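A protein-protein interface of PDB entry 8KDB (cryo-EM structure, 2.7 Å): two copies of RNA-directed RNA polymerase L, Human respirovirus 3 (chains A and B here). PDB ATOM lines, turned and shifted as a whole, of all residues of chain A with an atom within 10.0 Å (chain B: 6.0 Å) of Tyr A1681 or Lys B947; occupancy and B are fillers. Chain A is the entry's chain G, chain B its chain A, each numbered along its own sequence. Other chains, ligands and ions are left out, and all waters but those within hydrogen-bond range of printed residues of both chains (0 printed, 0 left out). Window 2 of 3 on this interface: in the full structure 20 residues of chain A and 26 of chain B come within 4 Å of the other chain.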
ATOM      1  N   MET A1604       3.707   9.532  35.018  1.00  0.00           N
ATOM      2  CA  MET A1604       3.900  10.577  34.016  1.00  0.00           C
ATOM      3  C   MET A1604       5.195  11.339  34.261  1.00  0.00           C
ATOM      4  O   MET A1604       5.954  11.607  33.320  1.00  0.00           O
ATOM      5  CB  MET A1604       2.713  11.534  34.004  1.00  0.00           C
ATOM      6  CG  MET A1604       1.419  10.916  33.526  1.00  0.00           C
ATOM      7  SD  MET A1604       1.149  11.231  31.775  1.00  0.00           S
ATOM      8  CE  MET A1604      -0.578  10.801  31.634  1.00  0.00           C
ATOM      9  N   GLU A1606       7.912  10.293  35.877  1.00  0.00           N
ATOM     10  CA  GLU A1606       9.059   9.437  35.590  1.00  0.00           C
ATOM     11  C   GLU A1606       9.273   9.272  34.091  1.00  0.00           C
ATOM     12  O   GLU A1606      10.411   9.335  33.611  1.00  0.00           O
ATOM     13  CB  GLU A1606       8.886   8.072  36.258  1.00  0.00           C
ATOM     14  CG  GLU A1606       8.802   8.122  37.774  1.00  0.00           C
ATOM     15  CD  GLU A1606      10.122   8.477  38.431  1.00  0.00           C
ATOM     16  OE1 GLU A1606      11.158   8.496  37.735  1.00  0.00           O
ATOM     17  OE2 GLU A1606      10.124   8.738  39.653  1.00  0.00           O
ATOM     18  N   TRP A1607       8.195   9.060  33.335  1.00  0.00           N
ATOM     19  CA  TRP A1607       8.330   8.885  31.893  1.00  0.00           C
ATOM     20  C   TRP A1607       8.853  10.150  31.228  1.00  0.00           C
ATOM     21  O   TRP A1607       9.723  10.084  30.353  1.00  0.00           O
ATOM     22  CB  TRP A1607       6.993   8.474  31.280  1.00  0.00           C
ATOM     23  CG  TRP A1607       7.103   8.133  29.830  1.00  0.00           C
ATOM     24  CD1 TRP A1607       6.801   8.939  28.774  1.00  0.00           C
ATOM     25  CD2 TRP A1607       7.568   6.899  29.274  1.00  0.00           C
ATOM     26  NE1 TRP A1607       7.040   8.280  27.593  1.00  0.00           N
ATOM     27  CE2 TRP A1607       7.511   7.025  27.873  1.00  0.00           C
ATOM     28  CE3 TRP A1607       8.022   5.698  29.825  1.00  0.00           C
ATOM     29  CZ2 TRP A1607       7.893   5.998  27.016  1.00  0.00           C
ATOM     30  CZ3 TRP A1607       8.399   4.680  28.972  1.00  0.00           C
ATOM     31  CH2 TRP A1607       8.334   4.836  27.584  1.00  0.00           C
ATOM     32  N   LEU A1608       8.338  11.315  31.627  1.00  0.00           N
ATOM     33  CA  LEU A1608       8.821  12.560  31.042  1.00  0.00           C
ATOM     34  C   LEU A1608      10.253  12.870  31.451  1.00  0.00           C
ATOM     35  O   LEU A1608      10.957  13.565  30.711  1.00  0.00           O
ATOM     36  CB  LEU A1608       7.896  13.715  31.425  1.00  0.00           C
ATOM     37  CG  LEU A1608       6.521  13.682  30.758  1.00  0.00           C
ATOM     38  CD1 LEU A1608       5.744  14.946  31.069  1.00  0.00           C
ATOM     39  CD2 LEU A1608       6.657  13.488  29.257  1.00  0.00           C
ATOM     40  N   ASN A1609      10.703  12.375  32.602  1.00  0.00           N
ATOM     41  CA  ASN A1609      12.094  12.519  33.009  1.00  0.00           C
ATOM     42  C   ASN A1609      13.004  11.466  32.386  1.00  0.00           C
ATOM     43  O   ASN A1609      14.134  11.290  32.852  1.00  0.00           O
ATOM     44  CB  ASN A1609      12.206  12.471  34.534  1.00  0.00           C
ATOM     45  CG  ASN A1609      12.002  13.827  35.175  1.00  0.00           C
ATOM     46  OD1 ASN A1609      12.253  14.861  34.557  1.00  0.00           O
ATOM     47  ND2 ASN A1609      11.547  13.832  36.420  1.00  0.00           N
ATOM     48  N   GLY A1610      12.542  10.772  31.351  1.00  0.00           N
ATOM     49  CA  GLY A1610      13.360   9.795  30.651  1.00  0.00           C
ATOM     50  C   GLY A1610      13.736   8.559  31.443  1.00  0.00           C
ATOM     51  O   GLY A1610      14.895   8.131  31.398  1.00  0.00           O
ATOM     52  N   VAL A1611      12.783   7.970  32.161  1.00  0.00           N
ATOM     53  CA  VAL A1611      13.008   6.756  32.938  1.00  0.00           C
ATOM     54  C   VAL A1611      12.288   5.606  32.247  1.00  0.00           C
ATOM     55  O   VAL A1611      11.108   5.723  31.897  1.00  0.00           O
ATOM     56  CB  VAL A1611      12.531   6.917  34.391  1.00  0.00           C
ATOM     57  CG1 VAL A1611      12.678   5.608  35.150  1.00  0.00           C
ATOM     58  CG2 VAL A1611      13.306   8.027  35.081  1.00  0.00           C
ATOM     59  N   VAL A1640       1.955   6.943  23.451  1.00  0.00           N
ATOM     60  CA  VAL A1640       3.020   7.893  23.139  1.00  0.00           C
ATOM     61  C   VAL A1640       2.533   8.920  22.125  1.00  0.00           C
ATOM     62  O   VAL A1640       2.881  10.105  22.201  1.00  0.00           O
ATOM     63  CB  VAL A1640       4.273   7.145  22.645  1.00  0.00           C
ATOM     64  CG1 VAL A1640       5.224   8.092  21.930  1.00  0.00           C
ATOM     65  CG2 VAL A1640       4.974   6.468  23.811  1.00  0.00           C
ATOM     66  N   LEU A1643       0.448  11.370  24.141  1.00  0.00           N
ATOM     67  CA  LEU A1643       1.214  12.221  25.048  1.00  0.00           C
ATOM     68  C   LEU A1643       2.009  13.281  24.298  1.00  0.00           C
ATOM     69  O   LEU A1643       2.311  14.339  24.860  1.00  0.00           O
ATOM     70  CB  LEU A1643       2.144  11.362  25.905  1.00  0.00           C
ATOM     71  CG  LEU A1643       2.959  12.061  26.994  1.00  0.00           C
ATOM     72  CD1 LEU A1643       2.044  12.683  28.030  1.00  0.00           C
ATOM     73  CD2 LEU A1643       3.923  11.086  27.648  1.00  0.00           C
ATOM     74  N   ALA A1644       2.349  13.027  23.037  1.00  0.00           N
ATOM     75  CA  ALA A1644       3.104  13.982  22.236  1.00  0.00           C
ATOM     76  C   ALA A1644       2.225  15.057  21.616  1.00  0.00           C
ATOM     77  O   ALA A1644       2.751  15.940  20.929  1.00  0.00           O
ATOM     78  CB  ALA A1644       3.877  13.253  21.134  1.00  0.00           C
ATOM     79  N   GLU A1645       0.911  15.000  21.840  1.00  0.00           N
ATOM     80  CA  GLU A1645      -0.035  15.969  21.286  1.00  0.00           C
ATOM     81  C   GLU A1645       0.030  16.003  19.761  1.00  0.00           C
ATOM     82  O   GLU A1645      -0.067  17.064  19.140  1.00  0.00           O
ATOM     83  CB  GLU A1645       0.190  17.364  21.874  1.00  0.00           C
ATOM     84  CG  GLU A1645       0.207  17.397  23.393  1.00  0.00           C
ATOM     85  CD  GLU A1645       0.028  18.797  23.947  1.00  0.00           C
ATOM     86  OE1 GLU A1645      -0.912  19.493  23.511  1.00  0.00           O
ATOM     87  OE2 GLU A1645       0.827  19.199  24.820  1.00  0.00           O
ATOM     88  N   ILE A1646       0.195  14.831  19.151  1.00  0.00           N
ATOM     89  CA  ILE A1646       0.227  14.709  17.697  1.00  0.00           C
ATOM     90  C   ILE A1646      -0.818  13.695  17.255  1.00  0.00           C
ATOM     91  O   ILE A1646      -0.807  13.237  16.107  1.00  0.00           O
ATOM     92  CB  ILE A1646       1.626  14.307  17.196  1.00  0.00           C
ATOM     93  CG1 ILE A1646       1.972  12.895  17.671  1.00  0.00           C
ATOM     94  CG2 ILE A1646       2.671  15.307  17.661  1.00  0.00           C
ATOM     95  CD1 ILE A1646       3.405  12.497  17.409  1.00  0.00           C
ATOM     96  N   ASN A1672       6.420  11.668  11.595  1.00  0.00           N
ATOM     97  CA  ASN A1672       6.532  12.837  12.464  1.00  0.00           C
ATOM     98  C   ASN A1672       7.973  13.072  12.899  1.00  0.00           C
ATOM     99  O   ASN A1672       8.424  14.220  12.977  1.00  0.00           O
ATOM    100  CB  ASN A1672       5.616  12.688  13.674  1.00  0.00           C
ATOM    101  CG  ASN A1672       4.181  13.020  13.348  1.00  0.00           C
ATOM    102  OD1 ASN A1672       3.311  12.159  13.394  1.00  0.00           O
ATOM    103  ND2 ASN A1672       3.927  14.279  13.011  1.00  0.00           N
ATOM    104  N   ILE A1673       8.713  11.999  13.183  1.00  0.00           N
ATOM    105  CA  ILE A1673      10.134  12.137  13.495  1.00  0.00           C
ATOM    106  C   ILE A1673      10.878  12.720  12.301  1.00  0.00           C
ATOM    107  O   ILE A1673      11.792  13.539  12.455  1.00  0.00           O
ATOM    108  CB  ILE A1673      10.716  10.778  13.926  1.00  0.00           C
ATOM    109  CG1 ILE A1673      10.227  10.406  15.326  1.00  0.00           C
ATOM    110  CG2 ILE A1673      12.238  10.798  13.878  1.00  0.00           C
ATOM    111  CD1 ILE A1673      10.987  11.086  16.440  1.00  0.00           C
ATOM    112  N   ASP A1676      10.217  16.711  12.416  1.00  0.00           N
ATOM    113  CA  ASP A1676      11.161  17.260  13.374  1.00  0.00           C
ATOM    114  C   ASP A1676      11.889  16.134  14.098  1.00  0.00           C
ATOM    115  O   ASP A1676      11.251  15.185  14.563  1.00  0.00           O
ATOM    116  CB  ASP A1676      10.466  18.174  14.401  1.00  0.00           C
ATOM    117  CG  ASP A1676       9.241  17.535  15.024  1.00  0.00           C
ATOM    118  OD1 ASP A1676       8.821  16.457  14.558  1.00  0.00           O
ATOM    119  OD2 ASP A1676       8.697  18.113  15.988  1.00  0.00           O
ATOM    120  N   PRO A1677      13.220  16.211  14.205  1.00  0.00           N
ATOM    121  CA  PRO A1677      13.974  15.078  14.774  1.00  0.00           C
ATOM    122  C   PRO A1677      13.521  14.682  16.167  1.00  0.00           C
ATOM    123  O   PRO A1677      13.525  13.490  16.501  1.00  0.00           O
ATOM    124  CB  PRO A1677      15.421  15.591  14.768  1.00  0.00           C
ATOM    125  CG  PRO A1677      15.447  16.637  13.702  1.00  0.00           C
ATOM    126  CD  PRO A1677      14.105  17.299  13.760  1.00  0.00           C
ATOM    127  N   THR A1678      13.127  15.648  16.992  1.00  0.00           N
ATOM    128  CA  THR A1678      12.562  15.383  18.307  1.00  0.00           C
ATOM    129  C   THR A1678      11.101  15.808  18.312  1.00  0.00           C
ATOM    130  O   THR A1678      10.789  16.971  18.036  1.00  0.00           O
ATOM    131  CB  THR A1678      13.332  16.131  19.396  1.00  0.00           C
ATOM    132  OG1 THR A1678      13.456  17.511  19.032  1.00  0.00           O
ATOM    133  CG2 THR A1678      14.718  15.533  19.573  1.00  0.00           C
ATOM    134  N   LEU A1679      10.209  14.867  18.628  1.00  0.00           N
ATOM    135  CA  LEU A1679       8.777  15.158  18.694  1.00  0.00           C
ATOM    136  C   LEU A1679       8.482  15.765  20.064  1.00  0.00           C
ATOM    137  O   LEU A1679       7.890  15.152  20.955  1.00  0.00           O
ATOM    138  CB  LEU A1679       7.956  13.905  18.391  1.00  0.00           C
ATOM    139  CG  LEU A1679       7.810  12.715  19.348  1.00  0.00           C
ATOM    140  CD1 LEU A1679       6.658  11.820  18.926  1.00  0.00           C
ATOM    141  CD2 LEU A1679       9.098  11.928  19.436  1.00  0.00           C
ATOM    142  N   LYS A1680       8.920  17.015  20.223  1.00  0.00           N
ATOM    143  CA  LYS A1680       8.802  17.749  21.482  1.00  0.00           C
ATOM    144  C   LYS A1680       9.540  17.043  22.616  1.00  0.00           C
ATOM    145  O   LYS A1680       9.148  17.137  23.781  1.00  0.00           O
ATOM    146  CB  LYS A1680       7.333  17.988  21.845  1.00  0.00           C
ATOM    147  CG  LYS A1680       6.520  18.546  20.688  1.00  0.00           C
ATOM    148  CD  LYS A1680       5.037  18.282  20.851  1.00  0.00           C
ATOM    149  CE  LYS A1680       4.271  18.732  19.618  1.00  0.00           C
ATOM    150  NZ  LYS A1680       2.806  18.515  19.752  1.00  0.00           N
ATOM    151  N   TYR A1681      10.615  16.330  22.266  1.00  0.00           N
ATOM    152  CA  TYR A1681      11.531  15.718  23.233  1.00  0.00           C
ATOM    153  C   TYR A1681      10.811  14.768  24.187  1.00  0.00           C
ATOM    154  O   TYR A1681      11.096  14.728  25.386  1.00  0.00           O
ATOM    155  CB  TYR A1681      12.305  16.787  24.009  1.00  0.00           C
ATOM    156  CG  TYR A1681      13.137  17.694  23.128  1.00  0.00           C
ATOM    157  CD1 TYR A1681      12.559  18.757  22.447  1.00  0.00           C
ATOM    158  CD2 TYR A1681      14.498  17.478  22.969  1.00  0.00           C
ATOM    159  CE1 TYR A1681      13.314  19.582  21.638  1.00  0.00           C
ATOM    160  CE2 TYR A1681      15.261  18.298  22.162  1.00  0.00           C
ATOM    161  CZ  TYR A1681      14.664  19.348  21.500  1.00  0.00           C
ATOM    162  OH  TYR A1681      15.422  20.166  20.696  1.00  0.00           O
ATOM    163  N   VAL A1682       9.877  13.986  23.652  1.00  0.00           N
ATOM    164  CA  VAL A1682       9.157  12.973  24.416  1.00  0.00           C
ATOM    165  C   VAL A1682       9.797  11.620  24.139  1.00  0.00           C
ATOM    166  O   VAL A1682      10.038  11.266  22.980  1.00  0.00           O
ATOM    167  CB  VAL A1682       7.662  12.963  24.056  1.00  0.00           C
ATOM    168  CG1 VAL A1682       6.944  11.836  24.782  1.00  0.00           C
ATOM    169  CG2 VAL A1682       7.028  14.304  24.391  1.00  0.00           C
ATOM    170  N   GLN A1683      10.080  10.870  25.201  1.00  0.00           N
ATOM    171  CA  GLN A1683      10.750   9.582  25.074  1.00  0.00           C
ATOM    172  C   GLN A1683       9.872   8.579  24.332  1.00  0.00           C
ATOM    173  O   GLN A1683       8.640   8.628  24.399  1.00  0.00           O
ATOM    174  CB  GLN A1683      11.113   9.041  26.457  1.00  0.00           C
ATOM    175  CG  GLN A1683      12.061   7.854  26.452  1.00  0.00           C
ATOM    176  CD  GLN A1683      11.991   7.054  27.738  1.00  0.00           C
ATOM    177  OE1 GLN A1683      10.996   7.104  28.459  1.00  0.00           O
ATOM    178  NE2 GLN A1683      13.052   6.313  28.032  1.00  0.00           N
ATOM    179  N   ILE A1684      10.520   7.659  23.615  1.00  0.00           N
ATOM    180  CA  ILE A1684       9.805   6.632  22.864  1.00  0.00           C
ATOM    181  C   ILE A1684      10.223   5.256  23.361  1.00  0.00           C
ATOM    182  O   ILE A1684       9.402   4.486  23.869  1.00  0.00           O
ATOM    183  CB  ILE A1684      10.064   6.735  21.349  1.00  0.00           C
ATOM    184  CG1 ILE A1684       9.618   8.087  20.793  1.00  0.00           C
ATOM    185  CG2 ILE A1684       9.358   5.606  20.615  1.00  0.00           C
ATOM    186  CD1 ILE A1684      10.720   9.120  20.799  1.00  0.00           C
ATOM    187  N   SER A1685      11.510   4.940  23.211  1.00  0.00           N
ATOM    188  CA  SER A1685      12.020   3.594  23.468  1.00  0.00           C
ATOM    189  C   SER A1685      12.424   3.458  24.937  1.00  0.00           C
ATOM    190  O   SER A1685      13.589   3.277  25.292  1.00  0.00           O
ATOM    191  CB  SER A1685      13.182   3.282  22.535  1.00  0.00           C
ATOM    192  OG  SER A1685      14.172   4.292  22.604  1.00  0.00           O
ATOM    193  N   GLN B 939      11.915  17.038  32.179  1.00  0.00           N
ATOM    194  CA  GLN B 939      13.068  17.246  31.313  1.00  0.00           C
ATOM    195  C   GLN B 939      12.678  17.685  29.910  1.00  0.00           C
ATOM    196  O   GLN B 939      13.419  18.447  29.278  1.00  0.00           O
ATOM    197  CB  GLN B 939      13.901  15.964  31.233  1.00  0.00           C
ATOM    198  CG  GLN B 939      15.195  16.106  30.456  1.00  0.00           C
ATOM    199  CD  GLN B 939      16.325  16.639  31.309  1.00  0.00           C
ATOM    200  OE1 GLN B 939      16.382  16.384  32.512  1.00  0.00           O
ATOM    201  NE2 GLN B 939      17.230  17.387  30.693  1.00  0.00           N
ATOM    202  N   ASN B 940      11.528  17.224  29.411  1.00  0.00           N
ATOM    203  CA  ASN B 940      11.113  17.587  28.061  1.00  0.00           C
ATOM    204  C   ASN B 940      10.876  19.088  27.937  1.00  0.00           C
ATOM    205  O   ASN B 940      11.316  19.710  26.967  1.00  0.00           O
ATOM    206  CB  ASN B 940       9.870  16.791  27.657  1.00  0.00           C
ATOM    207  CG  ASN B 940       8.646  17.163  28.462  1.00  0.00           C
ATOM    208  OD1 ASN B 940       8.681  17.183  29.692  1.00  0.00           O
ATOM    209  ND2 ASN B 940       7.550  17.453  27.772  1.00  0.00           N
ATOM    210  N   LYS B 942      12.262  21.383  29.848  1.00  0.00           N
ATOM    211  CA  LYS B 942      13.543  22.049  30.047  1.00  0.00           C
ATOM    212  C   LYS B 942      14.360  22.066  28.763  1.00  0.00           C
ATOM    213  O   LYS B 942      14.813  23.128  28.322  1.00  0.00           O
ATOM    214  CB  LYS B 942      14.320  21.371  31.174  1.00  0.00           C
ATOM    215  CG  LYS B 942      15.739  21.885  31.322  1.00  0.00           C
ATOM    216  CD  LYS B 942      16.502  21.140  32.400  1.00  0.00           C
ATOM    217  CE  LYS B 942      17.998  21.205  32.150  1.00  0.00           C
ATOM    218  NZ  LYS B 942      18.751  21.589  33.374  1.00  0.00           N
ATOM    219  N   ASP B 943      14.550  20.906  28.135  1.00  0.00           N
ATOM    220  CA  ASP B 943      15.350  20.903  26.916  1.00  0.00           C
ATOM    221  C   ASP B 943      14.596  21.451  25.712  1.00  0.00           C
ATOM    222  O   ASP B 943      15.240  21.911  24.764  1.00  0.00           O
ATOM    223  CB  ASP B 943      15.890  19.500  26.613  1.00  0.00           C
ATOM    224  CG  ASP B 943      14.828  18.432  26.670  1.00  0.00           C
ATOM    225  OD1 ASP B 943      13.682  18.704  26.269  1.00  0.00           O
ATOM    226  OD2 ASP B 943      15.143  17.311  27.121  1.00  0.00           O
ATOM    227  N   GLN B 944      13.260  21.454  25.736  1.00  0.00           N
ATOM    228  CA  GLN B 944      12.498  22.127  24.694  1.00  0.00           C
ATOM    229  C   GLN B 944      12.753  23.626  24.709  1.00  0.00           C
ATOM    230  O   GLN B 944      12.879  24.248  23.650  1.00  0.00           O
ATOM    231  CB  GLN B 944      11.010  21.837  24.879  1.00  0.00           C
ATOM    232  CG  GLN B 944      10.191  21.867  23.610  1.00  0.00           C
ATOM    233  CD  GLN B 944       8.760  21.439  23.849  1.00  0.00           C
ATOM    234  OE1 GLN B 944       8.402  21.027  24.950  1.00  0.00           O
ATOM    235  NE2 GLN B 944       7.933  21.537  22.817  1.00  0.00           N
ATOM    236  N   TYR B 945      12.828  24.222  25.898  1.00  0.00           N
ATOM    237  CA  TYR B 945      13.134  25.647  25.970  1.00  0.00           C
ATOM    238  C   TYR B 945      14.621  25.933  25.803  1.00  0.00           C
ATOM    239  O   TYR B 945      14.986  26.991  25.281  1.00  0.00           O
ATOM    240  CB  TYR B 945      12.635  26.232  27.289  1.00  0.00           C
ATOM    241  CG  TYR B 945      11.181  26.627  27.264  1.00  0.00           C
ATOM    242  CD1 TYR B 945      10.187  25.693  27.506  1.00  0.00           C
ATOM    243  CD2 TYR B 945      10.800  27.931  26.983  1.00  0.00           C
ATOM    244  CE1 TYR B 945       8.859  26.045  27.480  1.00  0.00           C
ATOM    245  CE2 TYR B 945       9.471  28.293  26.956  1.00  0.00           C
ATOM    246  CZ  TYR B 945       8.505  27.345  27.205  1.00  0.00           C
ATOM    247  OH  TYR B 945       7.176  27.692  27.179  1.00  0.00           O
ATOM    248  N   PHE B 946      15.490  25.018  26.239  1.00  0.00           N
ATOM    249  CA  PHE B 946      16.928  25.245  26.152  1.00  0.00           C
ATOM    250  C   PHE B 946      17.494  24.988  24.763  1.00  0.00           C
ATOM    251  O   PHE B 946      18.578  25.493  24.454  1.00  0.00           O
ATOM    252  CB  PHE B 946      17.667  24.359  27.156  1.00  0.00           C
ATOM    253  CG  PHE B 946      17.708  24.914  28.549  1.00  0.00           C
ATOM    254  CD1 PHE B 946      16.857  25.933  28.935  1.00  0.00           C
ATOM    255  CD2 PHE B 946      18.604  24.412  29.477  1.00  0.00           C
ATOM    256  CE1 PHE B 946      16.899  26.439  30.217  1.00  0.00           C
ATOM    257  CE2 PHE B 946      18.649  24.914  30.757  1.00  0.00           C
ATOM    258  CZ  PHE B 946      17.796  25.927  31.128  1.00  0.00           C
ATOM    259  N   LYS B 947      16.801  24.225  23.920  1.00  0.00           N
ATOM    260  CA  LYS B 947      17.358  23.818  22.638  1.00  0.00           C
ATOM    261  C   LYS B 947      16.670  24.444  21.436  1.00  0.00           C
ATOM    262  O   LYS B 947      17.331  24.675  20.423  1.00  0.00           O
ATOM    263  CB  LYS B 947      17.311  22.293  22.504  1.00  0.00           C
ATOM    264  CG  LYS B 947      18.223  21.579  23.488  1.00  0.00           C
ATOM    265  CD  LYS B 947      18.000  20.080  23.476  1.00  0.00           C
ATOM    266  CE  LYS B 947      19.191  19.351  24.069  1.00  0.00           C
ATOM    267  NZ  LYS B 947      19.788  20.112  25.199  1.00  0.00           N
ATOM    268  N   ASN B 948      15.371  24.717  21.512  1.00  0.00           N
ATOM    269  CA  ASN B 948      14.709  25.432  20.431  1.00  0.00           C
ATOM    270  C   ASN B 948      15.259  26.849  20.334  1.00  0.00           C
ATOM    271  O   ASN B 948      15.432  27.537  21.343  1.00  0.00           O
ATOM    272  CB  ASN B 948      13.198  25.457  20.653  1.00  0.00           C
ATOM    273  CG  ASN B 948      12.539  24.140  20.308  1.00  0.00           C
ATOM    274  OD1 ASN B 948      12.861  23.521  19.296  1.00  0.00           O
ATOM    275  ND2 ASN B 948      11.612  23.703  21.148  1.00  0.00           N
ATOM    276  N   SER B 949      15.538  27.281  19.108  1.00  0.00           N
ATOM    277  CA  SER B 949      16.213  28.554  18.896  1.00  0.00           C
ATOM    278  C   SER B 949      15.311  29.718  19.277  1.00  0.00           C
ATOM    279  O   SER B 949      14.125  29.739  18.932  1.00  0.00           O
ATOM    280  CB  SER B 949      16.648  28.681  17.438  1.00  0.00           C
ATOM    281  OG  SER B 949      15.529  28.626  16.571  1.00  0.00           O
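The backbone NH of Gln B939 is in hydrogen-bond range of the side-chain amide oxygen of Asn A1609, at 3.2 Å.
The backbone carbonyl oxygen (O) of Asn B940 sits close to the side-chain carboxylate (OD1) of Asp B943 (2.7 Å).
The backbone carbonyl oxygen of Gln B944 sits at hydrogen-bond distance from the side-chain amide nitrogen of Asn B948 (2.9 Å).
O of Ala A1644 is in hydrogen-bond range of NZ of Lys A1680, at 2.8 Å.
O of Glu A1645 sits at hydrogen-bond distance from NZ of Lys A1680, 3.3 Å away.
Among the printed residues, pairs that only touch across the chains: Tyr A1681 with Asp B943 (3.3 Å), Tyr A1681 with Asn B940 (3.3 Å), Tyr A1681 with Lys B947 (3.4 Å), Lys A1680 with Gln B944 (3.7 Å), Leu A1608 with Gln B939 (3.8 Å), Leu A1608 with Asn B940 (3.9 Å) and Lys A1680 with Asn B940 (3.96 Å).
Of the printed residues of chain B, Leu A1608 touches Gln B939 (3.8 Å) and Asn B940 (3.9 Å).
Printed residues of chain B within 4 Å of Lys A1680: Asn B940 and Gln B944.
Of the printed residues of chain A, Gln B939 touches Leu A1608 (3.8 Å) and Asn A1609 (3.2 Å).
Asn B940 touches just these residues of chain A: Leu A1608, Lys A1680 and Tyr A1681.
Gln B944 touches just one residue of chain A: Lys A1680 (3.7 Å).
The nearest printed residue of chain B that does not touch Leu A1608 is Asp B943 (6.7 Å).
Hydrophobic or aromatic side chains of chain A within 4 Å of the printed part of chain B: Leu A1608 and Tyr A1681.
Among the printed residues, no Asp or Glu carboxylate lies within 4 Å of a Lys or Arg side-chain nitrogen of the other chain.
No position is printed for both chains.
Of the 8 pairs that touch across the chains among the printed residues, none has its exchanged pair printed and touching as well.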
